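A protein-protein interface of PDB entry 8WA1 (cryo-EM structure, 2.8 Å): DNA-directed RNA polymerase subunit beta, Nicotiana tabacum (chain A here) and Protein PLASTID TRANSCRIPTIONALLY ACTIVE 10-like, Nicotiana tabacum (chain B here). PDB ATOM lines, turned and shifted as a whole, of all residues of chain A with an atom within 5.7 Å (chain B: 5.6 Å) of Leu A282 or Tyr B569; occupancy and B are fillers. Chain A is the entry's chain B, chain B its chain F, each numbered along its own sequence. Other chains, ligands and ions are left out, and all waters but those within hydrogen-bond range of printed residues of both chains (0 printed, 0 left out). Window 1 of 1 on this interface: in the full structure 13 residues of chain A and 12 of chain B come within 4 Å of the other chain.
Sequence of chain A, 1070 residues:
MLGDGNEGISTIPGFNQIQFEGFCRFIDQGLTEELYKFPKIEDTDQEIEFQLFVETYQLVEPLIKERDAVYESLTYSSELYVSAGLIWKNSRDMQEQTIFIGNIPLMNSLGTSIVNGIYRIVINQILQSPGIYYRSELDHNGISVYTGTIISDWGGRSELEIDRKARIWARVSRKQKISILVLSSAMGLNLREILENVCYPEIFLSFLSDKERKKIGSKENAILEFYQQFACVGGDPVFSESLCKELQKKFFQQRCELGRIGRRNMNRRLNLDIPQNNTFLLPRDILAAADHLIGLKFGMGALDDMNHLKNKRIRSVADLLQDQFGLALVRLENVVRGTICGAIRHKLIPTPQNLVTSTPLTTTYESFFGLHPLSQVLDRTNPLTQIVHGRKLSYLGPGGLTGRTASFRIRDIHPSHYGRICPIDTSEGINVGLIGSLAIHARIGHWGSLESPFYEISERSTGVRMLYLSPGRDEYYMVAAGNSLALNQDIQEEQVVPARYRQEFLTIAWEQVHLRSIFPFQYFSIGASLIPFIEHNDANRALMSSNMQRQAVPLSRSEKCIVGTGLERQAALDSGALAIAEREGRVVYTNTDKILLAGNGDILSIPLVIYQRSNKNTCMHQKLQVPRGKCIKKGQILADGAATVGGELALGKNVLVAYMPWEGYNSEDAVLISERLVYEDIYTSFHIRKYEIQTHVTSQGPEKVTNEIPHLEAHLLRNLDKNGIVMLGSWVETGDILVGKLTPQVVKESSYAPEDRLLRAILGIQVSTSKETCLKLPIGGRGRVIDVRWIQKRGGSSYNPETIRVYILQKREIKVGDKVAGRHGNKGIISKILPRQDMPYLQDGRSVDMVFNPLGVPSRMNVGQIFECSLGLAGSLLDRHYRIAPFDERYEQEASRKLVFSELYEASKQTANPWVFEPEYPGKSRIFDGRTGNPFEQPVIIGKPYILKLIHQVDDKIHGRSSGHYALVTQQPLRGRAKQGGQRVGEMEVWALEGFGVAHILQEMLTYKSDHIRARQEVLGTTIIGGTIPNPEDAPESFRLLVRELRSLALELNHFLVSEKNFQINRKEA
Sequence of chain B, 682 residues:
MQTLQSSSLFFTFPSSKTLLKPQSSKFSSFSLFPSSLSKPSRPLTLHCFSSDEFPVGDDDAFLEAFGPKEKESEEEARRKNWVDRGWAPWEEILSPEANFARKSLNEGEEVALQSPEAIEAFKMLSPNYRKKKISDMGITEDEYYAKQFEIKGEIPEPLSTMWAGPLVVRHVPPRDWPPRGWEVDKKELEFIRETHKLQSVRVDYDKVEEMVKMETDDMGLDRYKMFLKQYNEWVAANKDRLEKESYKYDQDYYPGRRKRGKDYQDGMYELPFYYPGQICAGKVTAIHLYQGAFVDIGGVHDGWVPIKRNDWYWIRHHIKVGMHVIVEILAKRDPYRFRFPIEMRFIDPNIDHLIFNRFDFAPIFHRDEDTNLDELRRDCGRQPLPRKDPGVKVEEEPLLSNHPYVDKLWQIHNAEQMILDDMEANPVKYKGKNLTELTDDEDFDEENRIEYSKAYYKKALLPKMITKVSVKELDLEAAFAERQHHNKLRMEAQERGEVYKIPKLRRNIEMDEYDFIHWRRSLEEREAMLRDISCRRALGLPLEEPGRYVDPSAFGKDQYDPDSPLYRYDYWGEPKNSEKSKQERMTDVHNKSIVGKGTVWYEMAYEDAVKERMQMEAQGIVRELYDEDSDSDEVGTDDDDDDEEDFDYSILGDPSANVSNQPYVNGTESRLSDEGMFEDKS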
ATOM      1  N   ARG A 263       9.114   2.935  24.438  1.00  0.00           N
ATOM      2  CA  ARG A 263       9.110   3.837  25.557  1.00  0.00           C
ATOM      3  C   ARG A 263      10.485   3.900  26.136  1.00  0.00           C
ATOM      4  O   ARG A 263      10.989   4.976  26.414  1.00  0.00           O
ATOM      5  CB  ARG A 263       8.159   3.319  26.621  1.00  0.00           C
ATOM      6  CG  ARG A 263       8.190   4.051  27.954  1.00  0.00           C
ATOM      7  CD  ARG A 263       7.380   5.332  27.904  1.00  0.00           C
ATOM      8  NE  ARG A 263       8.135   6.438  27.332  1.00  0.00           N
ATOM      9  CZ  ARG A 263       7.591   7.568  26.901  1.00  0.00           C
ATOM     10  NH1 ARG A 263       6.279   7.743  26.964  1.00  0.00           N
ATOM     11  NH2 ARG A 263       8.360   8.517  26.397  1.00  0.00           N
ATOM     12  N   ILE A 274       9.541   9.175  32.369  1.00  0.00           N
ATOM     13  CA  ILE A 274       8.204   8.649  32.177  1.00  0.00           C
ATOM     14  C   ILE A 274       8.242   7.189  32.560  1.00  0.00           C
ATOM     15  O   ILE A 274       9.151   6.467  32.166  1.00  0.00           O
ATOM     16  CB  ILE A 274       7.782   8.750  30.708  1.00  0.00           C
ATOM     17  CG1 ILE A 274       8.137  10.124  30.138  1.00  0.00           C
ATOM     18  CG2 ILE A 274       6.304   8.442  30.540  1.00  0.00           C
ATOM     19  CD1 ILE A 274       7.368  11.261  30.766  1.00  0.00           C
ATOM     20  N   ASN A 277       5.416   1.852  32.216  1.00  0.00           N
ATOM     21  CA  ASN A 277       4.055   1.452  31.920  1.00  0.00           C
ATOM     22  C   ASN A 277       3.349   2.361  30.932  1.00  0.00           C
ATOM     23  O   ASN A 277       2.583   1.882  30.102  1.00  0.00           O
ATOM     24  CB  ASN A 277       3.266   1.401  33.221  1.00  0.00           C
ATOM     25  CG  ASN A 277       1.894   0.782  33.050  1.00  0.00           C
ATOM     26  OD1 ASN A 277       1.683  -0.071  32.189  1.00  0.00           O
ATOM     27  ND2 ASN A 277       0.951   1.202  33.884  1.00  0.00           N
ATOM     28  N   ASN A 278       3.603   3.658  30.982  1.00  0.00           N
ATOM     29  CA  ASN A 278       2.847   4.568  30.134  1.00  0.00           C
ATOM     30  C   ASN A 278       3.390   4.569  28.740  1.00  0.00           C
ATOM     31  O   ASN A 278       4.090   5.489  28.344  1.00  0.00           O
ATOM     32  CB  ASN A 278       2.947   5.978  30.684  1.00  0.00           C
ATOM     33  CG  ASN A 278       2.534   6.068  32.138  1.00  0.00           C
ATOM     34  OD1 ASN A 278       2.086   5.089  32.732  1.00  0.00           O
ATOM     35  ND2 ASN A 278       2.682   7.251  32.719  1.00  0.00           N
ATOM     36  N   THR A 279       3.049   3.545  27.978  1.00  0.00           N
ATOM     37  CA  THR A 279       3.581   3.424  26.641  1.00  0.00           C
ATOM     38  C   THR A 279       2.783   4.202  25.640  1.00  0.00           C
ATOM     39  O   THR A 279       2.183   3.627  24.738  1.00  0.00           O
ATOM     40  CB  THR A 279       3.559   1.959  26.194  1.00  0.00           C
ATOM     41  OG1 THR A 279       2.260   1.407  26.432  1.00  0.00           O
ATOM     42  CG2 THR A 279       4.586   1.154  26.969  1.00  0.00           C
ATOM     43  N   PHE A 280       2.798   5.514  25.766  1.00  0.00           N
ATOM     44  CA  PHE A 280       2.095   6.336  24.812  1.00  0.00           C
ATOM     45  C   PHE A 280       2.893   7.577  24.485  1.00  0.00           C
ATOM     46  O   PHE A 280       3.677   8.045  25.301  1.00  0.00           O
ATOM     47  CB  PHE A 280       0.724   6.700  25.350  1.00  0.00           C
ATOM     48  CG  PHE A 280      -0.270   5.590  25.239  1.00  0.00           C
ATOM     49  CD1 PHE A 280      -0.845   5.287  24.020  1.00  0.00           C
ATOM     50  CD2 PHE A 280      -0.611   4.834  26.344  1.00  0.00           C
ATOM     51  CE1 PHE A 280      -1.755   4.258  23.906  1.00  0.00           C
ATOM     52  CE2 PHE A 280      -1.520   3.805  26.240  1.00  0.00           C
ATOM     53  CZ  PHE A 280      -2.092   3.516  25.020  1.00  0.00           C
ATOM     54  N   LEU A 281       2.703   8.105  23.285  1.00  0.00           N
ATOM     55  CA  LEU A 281       3.439   9.284  22.881  1.00  0.00           C
ATOM     56  C   LEU A 281       2.922  10.484  23.640  1.00  0.00           C
ATOM     57  O   LEU A 281       1.975  11.136  23.214  1.00  0.00           O
ATOM     58  CB  LEU A 281       3.301   9.513  21.382  1.00  0.00           C
ATOM     59  CG  LEU A 281       4.115  10.635  20.743  1.00  0.00           C
ATOM     60  CD1 LEU A 281       5.586  10.501  21.100  1.00  0.00           C
ATOM     61  CD2 LEU A 281       3.920  10.615  19.236  1.00  0.00           C
ATOM     62  N   LEU A 282       3.536  10.779  24.775  1.00  0.00           N
ATOM     63  CA  LEU A 282       3.136  11.953  25.526  1.00  0.00           C
ATOM     64  C   LEU A 282       3.650  13.210  24.830  1.00  0.00           C
ATOM     65  O   LEU A 282       4.645  13.170  24.103  1.00  0.00           O
ATOM     66  CB  LEU A 282       3.665  11.867  26.956  1.00  0.00           C
ATOM     67  CG  LEU A 282       3.298  10.597  27.729  1.00  0.00           C
ATOM     68  CD1 LEU A 282       3.837  10.654  29.150  1.00  0.00           C
ATOM     69  CD2 LEU A 282       1.795  10.382  27.730  1.00  0.00           C
ATOM     70  N   PRO A 283       2.986  14.351  25.036  1.00  0.00           N
ATOM     71  CA  PRO A 283       3.470  15.603  24.435  1.00  0.00           C
ATOM     72  C   PRO A 283       4.778  16.099  25.024  1.00  0.00           C
ATOM     73  O   PRO A 283       5.488  16.863  24.352  1.00  0.00           O
ATOM     74  CB  PRO A 283       2.329  16.593  24.720  1.00  0.00           C
ATOM     75  CG  PRO A 283       1.135  15.742  25.024  1.00  0.00           C
ATOM     76  CD  PRO A 283       1.681  14.525  25.694  1.00  0.00           C
ATOM     77  N   ARG A 284       5.095  15.693  26.248  1.00  0.00           N
ATOM     78  CA  ARG A 284       6.370  16.072  26.842  1.00  0.00           C
ATOM     79  C   ARG A 284       7.475  15.462  26.009  1.00  0.00           C
ATOM     80  O   ARG A 284       8.517  16.074  25.803  1.00  0.00           O
ATOM     81  CB  ARG A 284       6.474  15.577  28.281  1.00  0.00           C
ATOM     82  CG  ARG A 284       7.814  15.859  28.946  1.00  0.00           C
ATOM     83  CD  ARG A 284       7.995  17.330  29.294  1.00  0.00           C
ATOM     84  NE  ARG A 284       8.723  18.080  28.274  1.00  0.00           N
ATOM     85  CZ  ARG A 284      10.036  18.287  28.293  1.00  0.00           C
ATOM     86  NH1 ARG A 284      10.773  17.799  29.282  1.00  0.00           N
ATOM     87  NH2 ARG A 284      10.613  18.986  27.327  1.00  0.00           N
ATOM     88  N   ASP A 285       7.245  14.249  25.521  1.00  0.00           N
ATOM     89  CA  ASP A 285       8.247  13.583  24.704  1.00  0.00           C
ATOM     90  C   ASP A 285       8.471  14.388  23.439  1.00  0.00           C
ATOM     91  O   ASP A 285       9.606  14.575  23.014  1.00  0.00           O
ATOM     92  CB  ASP A 285       7.788  12.174  24.336  1.00  0.00           C
ATOM     93  CG  ASP A 285       7.227  11.412  25.522  1.00  0.00           C
ATOM     94  OD1 ASP A 285       7.542  11.764  26.679  1.00  0.00           O
ATOM     95  OD2 ASP A 285       6.471  10.445  25.292  1.00  0.00           O
ATOM     96  N   ILE A 286       7.389  14.871  22.839  1.00  0.00           N
ATOM     97  CA  ILE A 286       7.504  15.692  21.640  1.00  0.00           C
ATOM     98  C   ILE A 286       8.232  16.993  21.949  1.00  0.00           C
ATOM     99  O   ILE A 286       9.068  17.445  21.169  1.00  0.00           O
ATOM    100  CB  ILE A 286       6.119  15.991  21.043  1.00  0.00           C
ATOM    101  CG1 ILE A 286       5.289  14.708  20.983  1.00  0.00           C
ATOM    102  CG2 ILE A 286       6.249  16.611  19.659  1.00  0.00           C
ATOM    103  CD1 ILE A 286       3.880  14.911  20.472  1.00  0.00           C
ATOM    104  N   LEU A 287       7.901  17.583  23.084  1.00  0.00           N
ATOM    105  CA  LEU A 287       8.526  18.835  23.463  1.00  0.00           C
ATOM    106  C   LEU A 287      10.006  18.611  23.595  1.00  0.00           C
ATOM    107  O   LEU A 287      10.809  19.387  23.094  1.00  0.00           O
ATOM    108  CB  LEU A 287       7.960  19.313  24.792  1.00  0.00           C
ATOM    109  CG  LEU A 287       8.217  20.767  25.179  1.00  0.00           C
ATOM    110  CD1 LEU A 287       7.644  21.698  24.122  1.00  0.00           C
ATOM    111  CD2 LEU A 287       7.609  21.068  26.539  1.00  0.00           C
ATOM    112  N   ASP B 563      -0.596  16.811  34.096  1.00  0.00           N
ATOM    113  CA  ASP B 563      -0.928  17.459  32.828  1.00  0.00           C
ATOM    114  C   ASP B 563      -0.317  18.853  32.730  1.00  0.00           C
ATOM    115  O   ASP B 563      -0.440  19.517  31.694  1.00  0.00           O
ATOM    116  CB  ASP B 563      -2.445  17.524  32.620  1.00  0.00           C
ATOM    117  CG  ASP B 563      -2.823  17.820  31.181  1.00  0.00           C
ATOM    118  OD1 ASP B 563      -2.635  16.933  30.324  1.00  0.00           O
ATOM    119  OD2 ASP B 563      -3.303  18.941  30.906  1.00  0.00           O
ATOM    120  N   LEU B 566       2.838  18.223  30.976  1.00  0.00           N
ATOM    121  CA  LEU B 566       2.355  17.401  29.866  1.00  0.00           C
ATOM    122  C   LEU B 566       2.776  15.943  30.040  1.00  0.00           C
ATOM    123  O   LEU B 566       3.190  15.276  29.090  1.00  0.00           O
ATOM    124  CB  LEU B 566       2.818  17.955  28.514  1.00  0.00           C
ATOM    125  CG  LEU B 566       1.993  19.066  27.852  1.00  0.00           C
ATOM    126  CD1 LEU B 566       1.686  20.208  28.810  1.00  0.00           C
ATOM    127  CD2 LEU B 566       2.718  19.595  26.626  1.00  0.00           C
ATOM    128  N   TYR B 567       2.666  15.447  31.270  1.00  0.00           N
ATOM    129  CA  TYR B 567       2.968  14.059  31.593  1.00  0.00           C
ATOM    130  C   TYR B 567       1.752  13.152  31.491  1.00  0.00           C
ATOM    131  O   TYR B 567       1.904  11.926  31.530  1.00  0.00           O
ATOM    132  CB  TYR B 567       3.559  13.959  33.003  1.00  0.00           C
ATOM    133  CG  TYR B 567       4.992  14.428  33.110  1.00  0.00           C
ATOM    134  CD1 TYR B 567       5.868  14.296  32.042  1.00  0.00           C
ATOM    135  CD2 TYR B 567       5.470  14.994  34.284  1.00  0.00           C
ATOM    136  CE1 TYR B 567       7.179  14.720  32.139  1.00  0.00           C
ATOM    137  CE2 TYR B 567       6.781  15.421  34.389  1.00  0.00           C
ATOM    138  CZ  TYR B 567       7.631  15.282  33.313  1.00  0.00           C
ATOM    139  OH  TYR B 567       8.935  15.707  33.413  1.00  0.00           O
ATOM    140  N   ARG B 568       0.555  13.718  31.364  1.00  0.00           N
ATOM    141  CA  ARG B 568      -0.654  12.920  31.239  1.00  0.00           C
ATOM    142  C   ARG B 568      -0.823  12.443  29.803  1.00  0.00           C
ATOM    143  O   ARG B 568      -0.217  12.988  28.876  1.00  0.00           O
ATOM    144  CB  ARG B 568      -1.878  13.728  31.670  1.00  0.00           C
ATOM    145  N   TYR B 569      -1.638  11.404  29.629  1.00  0.00           N
ATOM    146  CA  TYR B 569      -1.930  10.888  28.298  1.00  0.00           C
ATOM    147  C   TYR B 569      -2.525  11.983  27.423  1.00  0.00           C
ATOM    148  O   TYR B 569      -3.271  12.842  27.903  1.00  0.00           O
ATOM    149  CB  TYR B 569      -2.887   9.701  28.393  1.00  0.00           C
ATOM    150  CG  TYR B 569      -2.343   8.544  29.200  1.00  0.00           C
ATOM    151  CD1 TYR B 569      -1.507   7.599  28.619  1.00  0.00           C
ATOM    152  CD2 TYR B 569      -2.666   8.396  30.542  1.00  0.00           C
ATOM    153  CE1 TYR B 569      -1.008   6.540  29.352  1.00  0.00           C
ATOM    154  CE2 TYR B 569      -2.172   7.339  31.283  1.00  0.00           C
ATOM    155  CZ  TYR B 569      -1.344   6.415  30.682  1.00  0.00           C
ATOM    156  OH  TYR B 569      -0.849   5.361  31.415  1.00  0.00           O
ATOM    157  N   ASP B 570      -2.172  11.959  26.138  1.00  0.00           N
ATOM    158  CA  ASP B 570      -2.629  12.981  25.205  1.00  0.00           C
ATOM    159  C   ASP B 570      -4.150  13.083  25.208  1.00  0.00           C
ATOM    160  O   ASP B 570      -4.860  12.073  25.220  1.00  0.00           O
ATOM    161  CB  ASP B 570      -2.125  12.669  23.796  1.00  0.00           C
ATOM    162  N   TYR B 571      -4.648  14.317  25.203  1.00  0.00           N
ATOM    163  CA  TYR B 571      -6.087  14.576  25.234  1.00  0.00           C
ATOM    164  C   TYR B 571      -6.669  14.565  23.818  1.00  0.00           C
ATOM    165  O   TYR B 571      -7.321  15.505  23.368  1.00  0.00           O
ATOM    166  CB  TYR B 571      -6.370  15.896  25.942  1.00  0.00           C
ATOM    167  N   LYS B 580      -3.260   0.835  30.707  1.00  0.00           N
ATOM    168  CA  LYS B 580      -3.243   1.245  32.103  1.00  0.00           C
ATOM    169  C   LYS B 580      -4.610   1.777  32.504  1.00  0.00           C
ATOM    170  O   LYS B 580      -5.347   2.324  31.679  1.00  0.00           O
ATOM    171  CB  LYS B 580      -2.170   2.312  32.361  1.00  0.00           C
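Among the printed residues, merely in contact across the chains: Ile A274 with Tyr B567 (3.6 Å), Asn A277 with Lys B580 (3.6 Å), Phe A280 with Tyr B569 (3.5 Å), Leu A282 with Tyr B567 (3.3 Å), Leu A282 with Arg B568 (3.5 Å), Leu A282 with Tyr B569 (3.8 Å), Pro A283 with Leu B566 (3.6 Å) and Arg A284 with Tyr B567 (3.4 Å).
O of Asn A278 sits close to NH1 of Arg A263, 3.4 Å away. O of Phe A280 lies within hydrogen-bond range of NH1 of Arg A263 (3.1 Å). The side-chain carboxylate (OD2) of Asp A285 lies within hydrogen-bond range of the backbone NH (N) of Leu A282.
Printed residues of chain B within 4 Å of Asn A277: Lys B580 (3.6 Å). Of the printed residues of chain B, Phe A280 touches Tyr B569 (3.5 Å). Of the printed residues of chain B, Arg A284 touches Leu B566 (3.4 Å) and Tyr B567 (3.4 Å). Of the printed residues of chain A, Leu B566 touches Pro A283 and Arg A284. Of the printed residues of chain A, Tyr B567 touches Ile A274, Leu A282 and Arg A284. Tyr B569 touches just these residues of chain A: Asn A278 (3.2 Å), Phe A280 (3.5 Å) and Leu A282 (3.8 Å). The nearest residue of chain A that does not touch Tyr B569 is Asn A277 (5.1 Å).
OD1 of Asn A278 lies within hydrogen-bond range of OH of Tyr B569 (3.2 Å). The backbone carbonyl oxygen of Leu B566 sits close to the backbone NH of Arg A284 (3.4 Å).
Of the 8 printed residues of chain B, 5 touch a printed residue of chain A. Hydrophobic or aromatic side chains of chain B within 4 Å of the printed part of chain A: Leu B566, Tyr B567 and Tyr B569. Among the printed residues, 10 pairs touch across the chains. Among the printed residues, no Asp or Glu carboxylate lies within 4 Å of a Lys or Arg side-chain nitrogen of the other chain.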
